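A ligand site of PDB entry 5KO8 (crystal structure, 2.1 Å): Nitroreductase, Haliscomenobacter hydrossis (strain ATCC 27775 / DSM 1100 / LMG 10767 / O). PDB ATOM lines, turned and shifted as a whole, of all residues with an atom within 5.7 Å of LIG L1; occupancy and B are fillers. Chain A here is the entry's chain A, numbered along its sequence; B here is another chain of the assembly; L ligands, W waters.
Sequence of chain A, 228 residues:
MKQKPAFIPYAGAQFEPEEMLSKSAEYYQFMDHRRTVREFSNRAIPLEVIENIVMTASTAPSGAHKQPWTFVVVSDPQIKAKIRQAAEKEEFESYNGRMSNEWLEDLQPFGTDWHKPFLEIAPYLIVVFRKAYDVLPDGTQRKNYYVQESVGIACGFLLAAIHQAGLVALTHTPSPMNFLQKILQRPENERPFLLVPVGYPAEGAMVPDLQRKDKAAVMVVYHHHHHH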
ATOM      1  N   ARG A  34      22.048  -2.148 -20.023  1.00  0.00           N
ATOM      2  CA  ARG A  34      21.810  -2.760 -18.728  1.00  0.00           C
ATOM      3  C   ARG A  34      21.167  -1.741 -17.804  1.00  0.00           C
ATOM      4  O   ARG A  34      21.599  -0.588 -17.742  1.00  0.00           O
ATOM      5  CB  ARG A  34      23.106  -3.275 -18.102  1.00  0.00           C
ATOM      6  CG  ARG A  34      22.894  -4.027 -16.785  1.00  0.00           C
ATOM      7  CD  ARG A  34      24.088  -3.890 -15.858  1.00  0.00           C
ATOM      8  NE  ARG A  34      24.327  -2.505 -15.494  1.00  0.00           N
ATOM      9  CZ  ARG A  34      23.689  -1.854 -14.532  1.00  0.00           C
ATOM     10  NH1 ARG A  34      22.763  -2.471 -13.802  1.00  0.00           N
ATOM     11  NH2 ARG A  34      23.970  -0.588 -14.287  1.00  0.00           N
ATOM     12  N   ARG A  35      20.135  -2.187 -17.090  1.00  0.00           N
ATOM     13  CA  ARG A  35      19.499  -1.383 -16.062  1.00  0.00           C
ATOM     14  C   ARG A  35      19.107  -2.258 -14.885  1.00  0.00           C
ATOM     15  O   ARG A  35      18.736  -3.410 -15.044  1.00  0.00           O
ATOM     16  CB  ARG A  35      18.271  -0.649 -16.604  1.00  0.00           C
ATOM     17  CG  ARG A  35      18.568   0.417 -17.679  1.00  0.00           C
ATOM     18  CD  ARG A  35      19.318   1.605 -17.099  1.00  0.00           C
ATOM     19  NE  ARG A  35      18.666   2.116 -15.904  1.00  0.00           N
ATOM     20  CZ  ARG A  35      17.704   3.043 -15.896  1.00  0.00           C
ATOM     21  NH1 ARG A  35      17.280   3.587 -17.031  1.00  0.00           N
ATOM     22  NH2 ARG A  35      17.165   3.416 -14.740  1.00  0.00           N
ATOM     23  N   THR A  36      19.228  -1.702 -13.680  1.00  0.00           N
ATOM     24  CA  THR A  36      18.751  -2.387 -12.497  1.00  0.00           C
ATOM     25  C   THR A  36      17.243  -2.558 -12.613  1.00  0.00           C
ATOM     26  O   THR A  36      16.521  -1.597 -12.889  1.00  0.00           O
ATOM     27  CB  THR A  36      19.108  -1.591 -11.226  1.00  0.00           C
ATOM     28  OG1 THR A  36      20.532  -1.463 -11.133  1.00  0.00           O
ATOM     29  CG2 THR A  36      18.587  -2.284  -9.978  1.00  0.00           C
ATOM     30  N   ARG A  38      13.725  -4.111 -10.791  1.00  0.00           N
ATOM     31  CA  ARG A  38      13.181  -4.441  -9.480  1.00  0.00           C
ATOM     32  C   ARG A  38      11.895  -5.273  -9.564  1.00  0.00           C
ATOM     33  O   ARG A  38      11.387  -5.724  -8.541  1.00  0.00           O
ATOM     34  CB  ARG A  38      12.938  -3.163  -8.678  1.00  0.00           C
ATOM     35  CG  ARG A  38      14.220  -2.359  -8.466  1.00  0.00           C
ATOM     36  CD  ARG A  38      14.032  -1.169  -7.547  1.00  0.00           C
ATOM     37  NE  ARG A  38      15.309  -0.525  -7.237  1.00  0.00           N
ATOM     38  CZ  ARG A  38      15.933   0.333  -8.035  1.00  0.00           C
ATOM     39  NH1 ARG A  38      15.418   0.663  -9.208  1.00  0.00           N
ATOM     40  NH2 ARG A  38      17.095   0.867  -7.654  1.00  0.00           N
ATOM     41  N   GLU A  91      14.134  -2.558   6.743  1.00  0.00           N
ATOM     42  CA  GLU A  91      13.857  -1.390   5.915  1.00  0.00           C
ATOM     43  C   GLU A  91      12.705  -0.575   6.447  1.00  0.00           C
ATOM     44  O   GLU A  91      12.682   0.641   6.306  1.00  0.00           O
ATOM     45  CB  GLU A  91      13.552  -1.824   4.489  1.00  0.00           C
ATOM     46  CG  GLU A  91      14.701  -2.514   3.840  1.00  0.00           C
ATOM     47  CD  GLU A  91      15.682  -1.561   3.199  1.00  0.00           C
ATOM     48  OE1 GLU A  91      15.789  -0.403   3.676  1.00  0.00           O
ATOM     49  OE2 GLU A  91      16.345  -1.969   2.225  1.00  0.00           O
ATOM     50  N   PHE A 110      13.579   6.707  -7.341  1.00  0.00           N
ATOM     51  CA  PHE A 110      13.555   5.268  -7.577  1.00  0.00           C
ATOM     52  C   PHE A 110      12.224   4.621  -7.199  1.00  0.00           C
ATOM     53  O   PHE A 110      11.923   3.516  -7.635  1.00  0.00           O
ATOM     54  CB  PHE A 110      14.694   4.602  -6.805  1.00  0.00           C
ATOM     55  CG  PHE A 110      16.026   5.258  -7.014  1.00  0.00           C
ATOM     56  CD1 PHE A 110      16.630   5.231  -8.258  1.00  0.00           C
ATOM     57  CD2 PHE A 110      16.655   5.919  -5.974  1.00  0.00           C
ATOM     58  CE1 PHE A 110      17.854   5.848  -8.454  1.00  0.00           C
ATOM     59  CE2 PHE A 110      17.879   6.536  -6.170  1.00  0.00           C
ATOM     60  CZ  PHE A 110      18.475   6.504  -7.411  1.00  0.00           C
ATOM     61  N   THR A 112      11.033   3.333  -4.419  1.00  0.00           N
ATOM     62  CA  THR A 112      11.103   2.103  -3.638  1.00  0.00           C
ATOM     63  C   THR A 112      10.480   2.281  -2.260  1.00  0.00           C
ATOM     64  O   THR A 112      10.670   3.309  -1.605  1.00  0.00           O
ATOM     65  CB  THR A 112      12.557   1.639  -3.467  1.00  0.00           C
ATOM     66  OG1 THR A 112      13.377   2.744  -3.066  1.00  0.00           O
ATOM     67  CG2 THR A 112      13.081   1.063  -4.766  1.00  0.00           C
ATOM     68  N   LYS A 116       9.583  -5.784  -0.673  1.00  0.00           N
ATOM     69  CA  LYS A 116      10.593  -6.503  -1.458  1.00  0.00           C
ATOM     70  C   LYS A 116      10.111  -7.855  -1.958  1.00  0.00           C
ATOM     71  O   LYS A 116      10.688  -8.885  -1.620  1.00  0.00           O
ATOM     72  CB  LYS A 116      11.839  -6.709  -0.616  1.00  0.00           C
ATOM     73  CG  LYS A 116      12.420  -5.428  -0.144  1.00  0.00           C
ATOM     74  CD  LYS A 116      13.791  -5.626   0.403  1.00  0.00           C
ATOM     75  CE  LYS A 116      14.217  -4.379   1.089  1.00  0.00           C
ATOM     76  NZ  LYS A 116      14.132  -3.168   0.210  1.00  0.00           N
ATOM     77  N   LEU A 170      19.044  -7.083  -9.504  1.00  0.00           N
ATOM     78  CA  LEU A 170      18.966  -5.932  -8.626  1.00  0.00           C
ATOM     79  C   LEU A 170      20.091  -6.027  -7.595  1.00  0.00           C
ATOM     80  O   LEU A 170      20.094  -6.903  -6.749  1.00  0.00           O
ATOM     81  CB  LEU A 170      17.604  -5.872  -7.936  1.00  0.00           C
ATOM     82  CG  LEU A 170      17.435  -4.940  -6.740  1.00  0.00           C
ATOM     83  CD1 LEU A 170      17.827  -3.519  -7.083  1.00  0.00           C
ATOM     84  CD2 LEU A 170      16.003  -4.994  -6.244  1.00  0.00           C
ATOM     85  N   THR A 171      21.059  -5.115  -7.693  1.00  0.00           N
ATOM     86  CA  THR A 171      22.135  -5.055  -6.716  1.00  0.00           C
ATOM     87  C   THR A 171      21.573  -4.472  -5.433  1.00  0.00           C
ATOM     88  O   THR A 171      21.143  -3.324  -5.409  1.00  0.00           O
ATOM     89  CB  THR A 171      23.314  -4.207  -7.229  1.00  0.00           C
ATOM     90  OG1 THR A 171      23.773  -4.735  -8.489  1.00  0.00           O
ATOM     91  CG2 THR A 171      24.457  -4.222  -6.240  1.00  0.00           C
ATOM     92  N   HIS A 172      21.552  -5.273  -4.373  1.00  0.00           N
ATOM     93  CA  HIS A 172      20.899  -4.876  -3.117  1.00  0.00           C
ATOM     94  C   HIS A 172      21.861  -4.934  -1.928  1.00  0.00           C
ATOM     95  O   HIS A 172      22.744  -5.793  -1.868  1.00  0.00           O
ATOM     96  CB  HIS A 172      19.683  -5.779  -2.868  1.00  0.00           C
ATOM     97  CG  HIS A 172      18.621  -5.147  -2.011  1.00  0.00           C
ATOM     98  ND1 HIS A 172      18.695  -5.147  -0.640  1.00  0.00           N
ATOM     99  CD2 HIS A 172      17.482  -4.506  -2.334  1.00  0.00           C
ATOM    100  CE1 HIS A 172      17.631  -4.527  -0.144  1.00  0.00           C
ATOM    101  NE2 HIS A 172      16.881  -4.124  -1.158  1.00  0.00           N
ATOM    102  N   THR A 173      21.682  -4.010  -0.985  1.00  0.00           N
ATOM    103  CA  THR A 173      22.494  -3.997   0.230  1.00  0.00           C
ATOM    104  C   THR A 173      22.316  -5.301   0.998  1.00  0.00           C
ATOM    105  O   THR A 173      21.225  -5.885   0.986  1.00  0.00           O
ATOM    106  CB  THR A 173      22.143  -2.825   1.154  1.00  0.00           C
ATOM    107  OG1 THR A 173      20.767  -2.899   1.538  1.00  0.00           O
ATOM    108  CG2 THR A 173      22.415  -1.502   0.458  1.00  0.00           C
ATOM    109  N   LEU A 194      26.999  -8.429  -0.686  1.00  0.00           N
ATOM    110  CA  LEU A 194      25.889  -7.981  -1.518  1.00  0.00           C
ATOM    111  C   LEU A 194      24.832  -9.045  -1.663  1.00  0.00           C
ATOM    112  O   LEU A 194      25.103 -10.245  -1.542  1.00  0.00           O
ATOM    113  CB  LEU A 194      26.371  -7.574  -2.919  1.00  0.00           C
ATOM    114  CG  LEU A 194      26.986  -6.186  -3.111  1.00  0.00           C
ATOM    115  CD1 LEU A 194      27.339  -6.027  -4.575  1.00  0.00           C
ATOM    116  CD2 LEU A 194      26.035  -5.093  -2.691  1.00  0.00           C
ATOM    117  N   LEU A 210      16.520   7.506 -15.602  1.00  0.00           N
ATOM    118  CA  LEU A 210      17.764   8.117 -15.146  1.00  0.00           C
ATOM    119  C   LEU A 210      18.707   8.385 -16.297  1.00  0.00           C
ATOM    120  O   LEU A 210      18.619   7.756 -17.354  1.00  0.00           O
ATOM    121  CB  LEU A 210      18.467   7.197 -14.150  1.00  0.00           C
ATOM    122  CG  LEU A 210      17.636   6.714 -12.979  1.00  0.00           C
ATOM    123  CD1 LEU A 210      18.419   5.673 -12.195  1.00  0.00           C
ATOM    124  CD2 LEU A 210      17.221   7.871 -12.081  1.00  0.00           C
ATOM    125  N   ARG A 212      22.919   8.729 -17.023  1.00  0.00           N
ATOM    126  CA  ARG A 212      24.257   8.517 -16.487  1.00  0.00           C
ATOM    127  C   ARG A 212      25.110   9.735 -16.774  1.00  0.00           C
ATOM    128  O   ARG A 212      24.812  10.509 -17.668  1.00  0.00           O
ATOM    129  CB  ARG A 212      24.869   7.250 -17.084  1.00  0.00           C
ATOM    130  CG  ARG A 212      24.230   5.973 -16.560  1.00  0.00           C
ATOM    131  CD  ARG A 212      24.715   4.727 -17.280  1.00  0.00           C
ATOM    132  NE  ARG A 212      24.127   3.542 -16.668  1.00  0.00           N
ATOM    133  CZ  ARG A 212      23.548   2.540 -17.332  1.00  0.00           C
ATOM    134  NH1 ARG A 212      23.503   2.545 -18.657  1.00  0.00           N
ATOM    135  NH2 ARG A 212      23.031   1.523 -16.651  1.00  0.00           N
ATOM    136  N   THR B  59      28.958   2.571 -16.678  1.00  0.00           N
ATOM    137  CA  THR B  59      27.568   2.120 -16.742  1.00  0.00           C
ATOM    138  C   THR B  59      27.178   1.248 -15.555  1.00  0.00           C
ATOM    139  O   THR B  59      26.042   0.776 -15.468  1.00  0.00           O
ATOM    140  CB  THR B  59      27.247   1.290 -18.009  1.00  0.00           C
ATOM    141  OG1 THR B  59      27.927   0.029 -17.945  1.00  0.00           O
ATOM    142  CG2 THR B  59      27.633   2.043 -19.273  1.00  0.00           C
ATOM    143  N   ALA B  60      28.128   1.012 -14.647  1.00  0.00           N
ATOM    144  CA  ALA B  60      27.886   0.141 -13.499  1.00  0.00           C
ATOM    145  C   ALA B  60      26.785   0.699 -12.610  1.00  0.00           C
ATOM    146  O   ALA B  60      26.529   1.897 -12.604  1.00  0.00           O
ATOM    147  CB  ALA B  60      29.156  -0.031 -12.695  1.00  0.00           C
ATOM    148  N   PRO B  61      26.118  -0.200 -11.855  1.00  0.00           N
ATOM    149  CA  PRO B  61      25.178   0.298 -10.857  1.00  0.00           C
ATOM    150  C   PRO B  61      25.935   1.006  -9.740  1.00  0.00           C
ATOM    151  O   PRO B  61      27.127   0.764  -9.573  1.00  0.00           O
ATOM    152  CB  PRO B  61      24.486  -0.973 -10.357  1.00  0.00           C
ATOM    153  CG  PRO B  61      25.515  -2.038 -10.545  1.00  0.00           C
ATOM    154  CD  PRO B  61      26.230  -1.672 -11.815  1.00  0.00           C
ATOM    155  N   SER B  62      25.253   1.860  -8.989  1.00  0.00           N
ATOM    156  CA  SER B  62      25.855   2.555  -7.869  1.00  0.00           C
ATOM    157  C   SER B  62      24.816   2.974  -6.837  1.00  0.00           C
ATOM    158  O   SER B  62      23.649   3.236  -7.187  1.00  0.00           O
ATOM    159  CB  SER B  62      26.629   3.790  -8.351  1.00  0.00           C
ATOM    160  OG  SER B  62      25.742   4.748  -8.906  1.00  0.00           O
ATOM    161  N   GLY B  63      25.224   3.036  -5.573  1.00  0.00           N
ATOM    162  CA  GLY B  63      24.323   3.438  -4.508  1.00  0.00           C
ATOM    163  C   GLY B  63      23.640   4.751  -4.803  1.00  0.00           C
ATOM    164  O   GLY B  63      24.315   5.781  -4.993  1.00  0.00           O
ATOM    165  N   ALA B  64      22.310   4.720  -4.882  1.00  0.00           N
ATOM    166  CA  ALA B  64      21.494   5.910  -5.111  1.00  0.00           C
ATOM    167  C   ALA B  64      21.842   6.612  -6.425  1.00  0.00           C
ATOM    168  O   ALA B  64      21.594   7.807  -6.592  1.00  0.00           O
ATOM    169  CB  ALA B  64      21.628   6.894  -3.958  1.00  0.00           C
ATOM    170  N   HIS B  65      22.427   5.853  -7.352  1.00  0.00           N
ATOM    171  CA  HIS B  65      22.824   6.393  -8.652  1.00  0.00           C
ATOM    172  C   HIS B  65      23.763   7.596  -8.511  1.00  0.00           C
ATOM    173  O   HIS B  65      23.668   8.563  -9.252  1.00  0.00           O
ATOM    174  CB  HIS B  65      21.577   6.794  -9.464  1.00  0.00           C
ATOM    175  CG  HIS B  65      21.869   7.169 -10.882  1.00  0.00           C
ATOM    176  ND1 HIS B  65      22.728   6.436 -11.687  1.00  0.00           N
ATOM    177  CD2 HIS B  65      21.462   8.218 -11.634  1.00  0.00           C
ATOM    178  CE1 HIS B  65      22.821   7.013 -12.867  1.00  0.00           C
ATOM    179  NE2 HIS B  65      22.056   8.098 -12.865  1.00  0.00           N
ATOM    180  N   TYR B 145      26.742   6.667  -0.851  1.00  0.00           N
ATOM    181  CA  TYR B 145      26.504   5.460  -0.073  1.00  0.00           C
ATOM    182  C   TYR B 145      27.026   4.206  -0.776  1.00  0.00           C
ATOM    183  O   TYR B 145      26.906   4.064  -1.993  1.00  0.00           O
ATOM    184  CB  TYR B 145      25.011   5.330   0.213  1.00  0.00           C
ATOM    185  CG  TYR B 145      24.426   6.601   0.793  1.00  0.00           C
ATOM    186  CD1 TYR B 145      24.571   6.889   2.149  1.00  0.00           C
ATOM    187  CD2 TYR B 145      23.746   7.512  -0.010  1.00  0.00           C
ATOM    188  CE1 TYR B 145      24.048   8.059   2.687  1.00  0.00           C
ATOM    189  CE2 TYR B 145      23.214   8.674   0.522  1.00  0.00           C
ATOM    190  CZ  TYR B 145      23.368   8.943   1.872  1.00  0.00           C
ATOM    191  OH  TYR B 145      22.850  10.102   2.402  1.00  0.00           O
ATOM    192  N   TYR B 146      27.602   3.319   0.029  1.00  0.00           N
ATOM    193  CA  TYR B 146      28.190   2.072  -0.443  1.00  0.00           C
ATOM    194  C   TYR B 146      29.150   2.354  -1.591  1.00  0.00           C
ATOM    195  O   TYR B 146      29.053   1.764  -2.670  1.00  0.00           O
ATOM    196  CB  TYR B 146      27.095   1.080  -0.841  1.00  0.00           C
ATOM    197  CG  TYR B 146      26.223   0.652   0.319  1.00  0.00           C
ATOM    198  CD1 TYR B 146      26.602  -0.404   1.143  1.00  0.00           C
ATOM    199  CD2 TYR B 146      25.038   1.307   0.612  1.00  0.00           C
ATOM    200  CE1 TYR B 146      25.822  -0.793   2.219  1.00  0.00           C
ATOM    201  CE2 TYR B 146      24.245   0.920   1.689  1.00  0.00           C
ATOM    202  CZ  TYR B 146      24.649  -0.134   2.486  1.00  0.00           C
ATOM    203  OH  TYR B 146      23.867  -0.527   3.553  1.00  0.00           O
ATOM    204  N   GLU B 149      31.700  -0.570  -2.595  1.00  0.00           N
ATOM    205  CA  GLU B 149      31.049  -1.611  -3.372  1.00  0.00           C
ATOM    206  C   GLU B 149      30.804  -1.157  -4.800  1.00  0.00           C
ATOM    207  O   GLU B 149      31.095  -1.876  -5.759  1.00  0.00           O
ATOM    208  CB  GLU B 149      29.722  -2.010  -2.715  1.00  0.00           C
ATOM    209  CG  GLU B 149      29.844  -2.682  -1.350  1.00  0.00           C
ATOM    210  CD  GLU B 149      30.064  -1.707  -0.189  1.00  0.00           C
ATOM    211  OE1 GLU B 149      30.084  -0.478  -0.418  1.00  0.00           O
ATOM    212  OE2 GLU B 149      30.205  -2.182   0.955  1.00  0.00           O
ATOM    213  N   SER B 150      30.273   0.060  -4.942  1.00  0.00           N
ATOM    214  CA  SER B 150      29.956   0.652  -6.232  1.00  0.00           C
ATOM    215  C   SER B 150      31.177   0.774  -7.128  1.00  0.00           C
ATOM    216  O   SER B 150      31.122   0.423  -8.308  1.00  0.00           O
ATOM    217  CB  SER B 150      29.333   2.035  -6.025  1.00  0.00           C
ATOM    218  OG  SER B 150      28.144   1.963  -5.249  1.00  0.00           O
ATOM    219  N   ILE B 153      32.588  -2.577  -8.253  1.00  0.00           N
ATOM    220  CA  ILE B 153      31.793  -3.131  -9.340  1.00  0.00           C
ATOM    221  C   ILE B 153      32.151  -2.448 -10.661  1.00  0.00           C
ATOM    222  O   ILE B 153      32.345  -3.121 -11.660  1.00  0.00           O
ATOM    223  CB  ILE B 153      30.271  -2.967  -9.052  1.00  0.00           C
ATOM    224  CG1 ILE B 153      29.838  -3.955  -7.968  1.00  0.00           C
ATOM    225  CG2 ILE B 153      29.430  -3.209 -10.302  1.00  0.00           C
ATOM    226  CD1 ILE B 153      28.461  -3.676  -7.392  1.00  0.00           C
HETATM  227  N1  LIG L   1      18.597  -0.542  -5.324  1.00  0.00           N
HETATM  228  C1  LIG L   1      17.534  -0.702  -4.445  1.00  0.00           C
HETATM  229  O1  LIG L   1      16.382  -0.579  -4.857  1.00  0.00           O
HETATM  230  N2  LIG L   1      17.773  -0.979  -3.118  1.00  0.00           N
HETATM  231  C2  LIG L   1      19.065  -1.115  -2.664  1.00  0.00           C
HETATM  232  O2  LIG L   1      19.261  -1.376  -1.474  1.00  0.00           O
HETATM  233  C3  LIG L   1      20.134  -0.964  -3.542  1.00  0.00           C
HETATM  234  N3  LIG L   1      21.436  -1.091  -3.081  1.00  0.00           N
HETATM  235  C4  LIG L   1      22.500  -0.942  -3.946  1.00  0.00           C
HETATM  236  C5  LIG L   1      23.800  -1.093  -3.466  1.00  0.00           C
HETATM  237  C6  LIG L   1      24.884  -0.951  -4.322  1.00  0.00           C
HETATM  238  C7  LIG L   1      26.279  -1.106  -3.773  1.00  0.00           C
HETATM  239  C8  LIG L   1      24.654  -0.658  -5.666  1.00  0.00           C
HETATM  240  C9  LIG L   1      25.793  -0.508  -6.621  1.00  0.00           C
HETATM  241  C10 LIG L   1      23.352  -0.520  -6.141  1.00  0.00           C
HETATM  242  C11 LIG L   1      22.261  -0.655  -5.286  1.00  0.00           C
HETATM  243  N4  LIG L   1      20.959  -0.517  -5.762  1.00  0.00           N
HETATM  244  C12 LIG L   1      19.896  -0.676  -4.882  1.00  0.00           C
HETATM  245  C13 LIG L   1      20.682  -0.216  -7.206  1.00  0.00           C
HETATM  246  C14 LIG L   1      20.938   1.254  -7.552  1.00  0.00           C
HETATM  247  O3  LIG L   1      19.937   2.067  -6.962  1.00  0.00           O
HETATM  248  C15 LIG L   1      20.980   1.450  -9.065  1.00  0.00           C
HETATM  249  O4  LIG L   1      22.115   0.762  -9.530  1.00  0.00           O
HETATM  250  C16 LIG L   1      21.010   2.916  -9.474  1.00  0.00           C
HETATM  251  O5  LIG L   1      19.766   3.519  -9.163  1.00  0.00           O
HETATM  252  C17 LIG L   1      21.312   3.123 -10.954  1.00  0.00           C
HETATM  253  O6  LIG L   1      20.431   2.381 -11.779  1.00  0.00           O
HETATM  254  P1  LIG L   1      21.056   1.454 -12.935  1.00  0.00           P
HETATM  255  O7  LIG L   1      19.906   0.872 -13.730  1.00  0.00           O
HETATM  256  O8  LIG L   1      21.840   0.351 -12.279  1.00  0.00           O
HETATM  257  O9  LIG L   1      21.971   2.258 -13.823  1.00  0.00           O
HETATM  258  N1  LG2 L   2      17.913  -0.536   0.611  1.00  0.00           N
HETATM  259  C1  LG2 L   2      16.791   0.380   0.524  1.00  0.00           C
HETATM  260  C2  LG2 L   2      17.129   1.859   0.235  1.00  0.00           C
HETATM  261  C3  LG2 L   2      17.988   2.068  -0.966  1.00  0.00           C
HETATM  262  C4  LG2 L   2      19.372   2.188  -0.831  1.00  0.00           C
HETATM  263  C5  LG2 L   2      20.205   2.394  -1.950  1.00  0.00           C
HETATM  264  I1  LG2 L   2      22.193   2.547  -1.619  1.00  0.00           I
HETATM  265  C6  LG2 L   2      19.622   2.478  -3.220  1.00  0.00           C
HETATM  266  O1  LG2 L   2      20.315   2.669  -4.394  1.00  0.00           O
HETATM  267  C7  LG2 L   2      18.223   2.357  -3.364  1.00  0.00           C
HETATM  268  C8  LG2 L   2      17.420   2.160  -2.252  1.00  0.00           C
HETATM  269  C9  LG2 L   2      15.802  -0.166  -0.497  1.00  0.00           C
HETATM  270  O2  LG2 L   2      15.885  -1.207  -1.157  1.00  0.00           O
HETATM  271  O3  LG2 L   2      14.681   0.593  -0.682  1.00  0.00           O
HETATM  272  O   HOH W   1      21.183   4.679 -14.626  1.00  0.00           O
HETATM  273  O   HOH W   2      24.633   3.453 -13.878  1.00  0.00           O
HETATM  274  O   HOH W   3      17.518   2.586 -10.349  1.00  0.00           O
HETATM  275  O   HOH W   4      14.288  -2.068  -3.715  1.00  0.00           O
HETATM  276  O   HOH W   5      24.546   4.379 -11.182  1.00  0.00           O
HETATM  277  O   HOH W   6      17.319   1.101 -12.822  1.00  0.00           O
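NH2 of Arg 34 lies within salt-bridge range of O8 of LIG L1.
The side-chain carboxylate (OE2) of Glu 91 is in salt-bridge range of a nitrogen (N1) of LG2 L2, at 2.7 Å.
OG1 of Thr 112 sits at hydrogen-bond distance from O3 of LG2 L2 (3.5 Å).
NE2 of His 172 lies within hydrogen-bond range of O2 of LG2 L2 (3.1 Å).
O4 of LIG L1 lies within hydrogen-bond range of N of Ser 62 of chain B, 3.4 Å away.
O2 of LG2 L2 lies within salt-bridge range of NZ of Lys 116.
The backbone NH of Thr 36 sits at hydrogen-bond distance from an oxygen (O7) of LIG L1 (2.7 Å).
The side-chain hydroxyl (OG1) of Thr 36 sits at hydrogen-bond distance from an oxygen (O8) of LIG L1, 2.5 Å away.
NE of Arg 35 lies within salt-bridge range of O7 of LIG L1 (2.8 Å).
An oxygen (O9) of LIG L1 lies within salt-bridge range of the guanidinium group of Arg 212.
An oxygen (O1) of LIG L1 is in hydrogen-bond range of the guanidinium group of Arg 38 (2.6 Å).
The backbone NH of Ala 64 of chain B is in hydrogen-bond range of an oxygen (O1) of LG2 L2 (2.9 Å).
NE2 of His 172 lies within hydrogen-bond range of NZ of Lys 116 (3.2 Å).
The backbone carbonyl oxygen (O) of Arg 34 sits at hydrogen-bond distance from the guanidinium group (NH2) of Arg 212.
O of Thr 59 of chain B is in hydrogen-bond range of NH2 of Arg 34, at 2.7 Å.
The guanidinium group of Arg 212 is in hydrogen-bond range of the backbone carbonyl oxygen of Thr 59 of chain B, 3.3 Å away.
The backbone carbonyl oxygen of Tyr 146 of chain B sits at hydrogen-bond distance from the side-chain hydroxyl of Ser 150 of chain B (2.7 Å).
The backbone NH of Gly 63 of chain B sits at hydrogen-bond distance from the side-chain hydroxyl of Ser 150 of chain B, 3.1 Å away.
Water W3 lies within hydrogen-bond range of an oxygen (O5) of LIG L1 (2.7 Å) and the guanidinium group (NH1) of Arg 38 (3.1 Å).
Water W6 lies within hydrogen-bond range of an oxygen (O7) of LIG L1 (2.8 Å), the backbone carbonyl oxygen of Thr 36 (2.8 Å) and the guanidinium group of Arg 35 (3.0 Å).
Water W4 bridges an oxygen (O1) of LIG L1 (2.8 Å) and an oxygen (O2) of LG2 L2 (3.1 Å).
Water W2 lies within hydrogen-bond range of O of Ala 60 of chain B (2.8 Å), NE of Arg 212 (2.8 Å), O9 of LIG L1 (2.9 Å) and O of Thr 59 of chain B (3.4 Å).
Water W5 lies within hydrogen-bond range of OG of Ser 62 of chain B (2.6 Å), ND1 of His 65 of chain B (2.8 Å) and O of Ala 60 of chain B (3.5 Å).
A nitrogen (N4) of LIG L1 sits close to the backbone carbonyl oxygen (O) of Thr 171, 2.8 Å away.
Phe 110 touches LIG L1.
Thr 112 touches LIG L1 (CG2 to O1, 3.7 Å).
Leu 170 touches LIG L1.
CD2 of His 172 touches N2 of LIG L1 (3.6 Å).
Thr 173 touches LIG L1 (N to N3, 3.6 Å).
Leu 210 touches LIG L1.
CB of Pro 61 of chain B touches O4 of LIG L1 (3.1 Å).
Gly 63 of chain B touches LIG L1 (N to C8, 3.7 Å).
His 65 of chain B touches LIG L1.
CB of Tyr 146 of chain B touches C7 of LIG L1, 3.7 Å away.
Glu 149 of chain B touches LIG L1 (CB to C7, 3.7 Å).
OG of Ser 150 of chain B touches C9 of LIG L1 (3.7 Å).
Hydrophobic or aromatic side chains that line LIG L1: Phe 110, Leu 170, His 172, Leu 210, Pro 61 of chain B, His 65 of chain B and Tyr 146 of chain B.
Within 4 Å of LIG L1: Arg 34, Arg 35, Thr 36, Arg 38, Phe 110, Thr 112, Leu 170, Thr 171, His 172, Thr 173, Leu 210, Arg 212, Pro 61 of chain B, Ser 62 of chain B, Gly 63 of chain B, His 65 of chain B, Tyr 146 of chain B, Glu 149 of chain B and Ser 150 of chain B.
O2 of LIG L1 is in hydrogen-bond range of N1 of LG2 L2 (2.6 Å).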
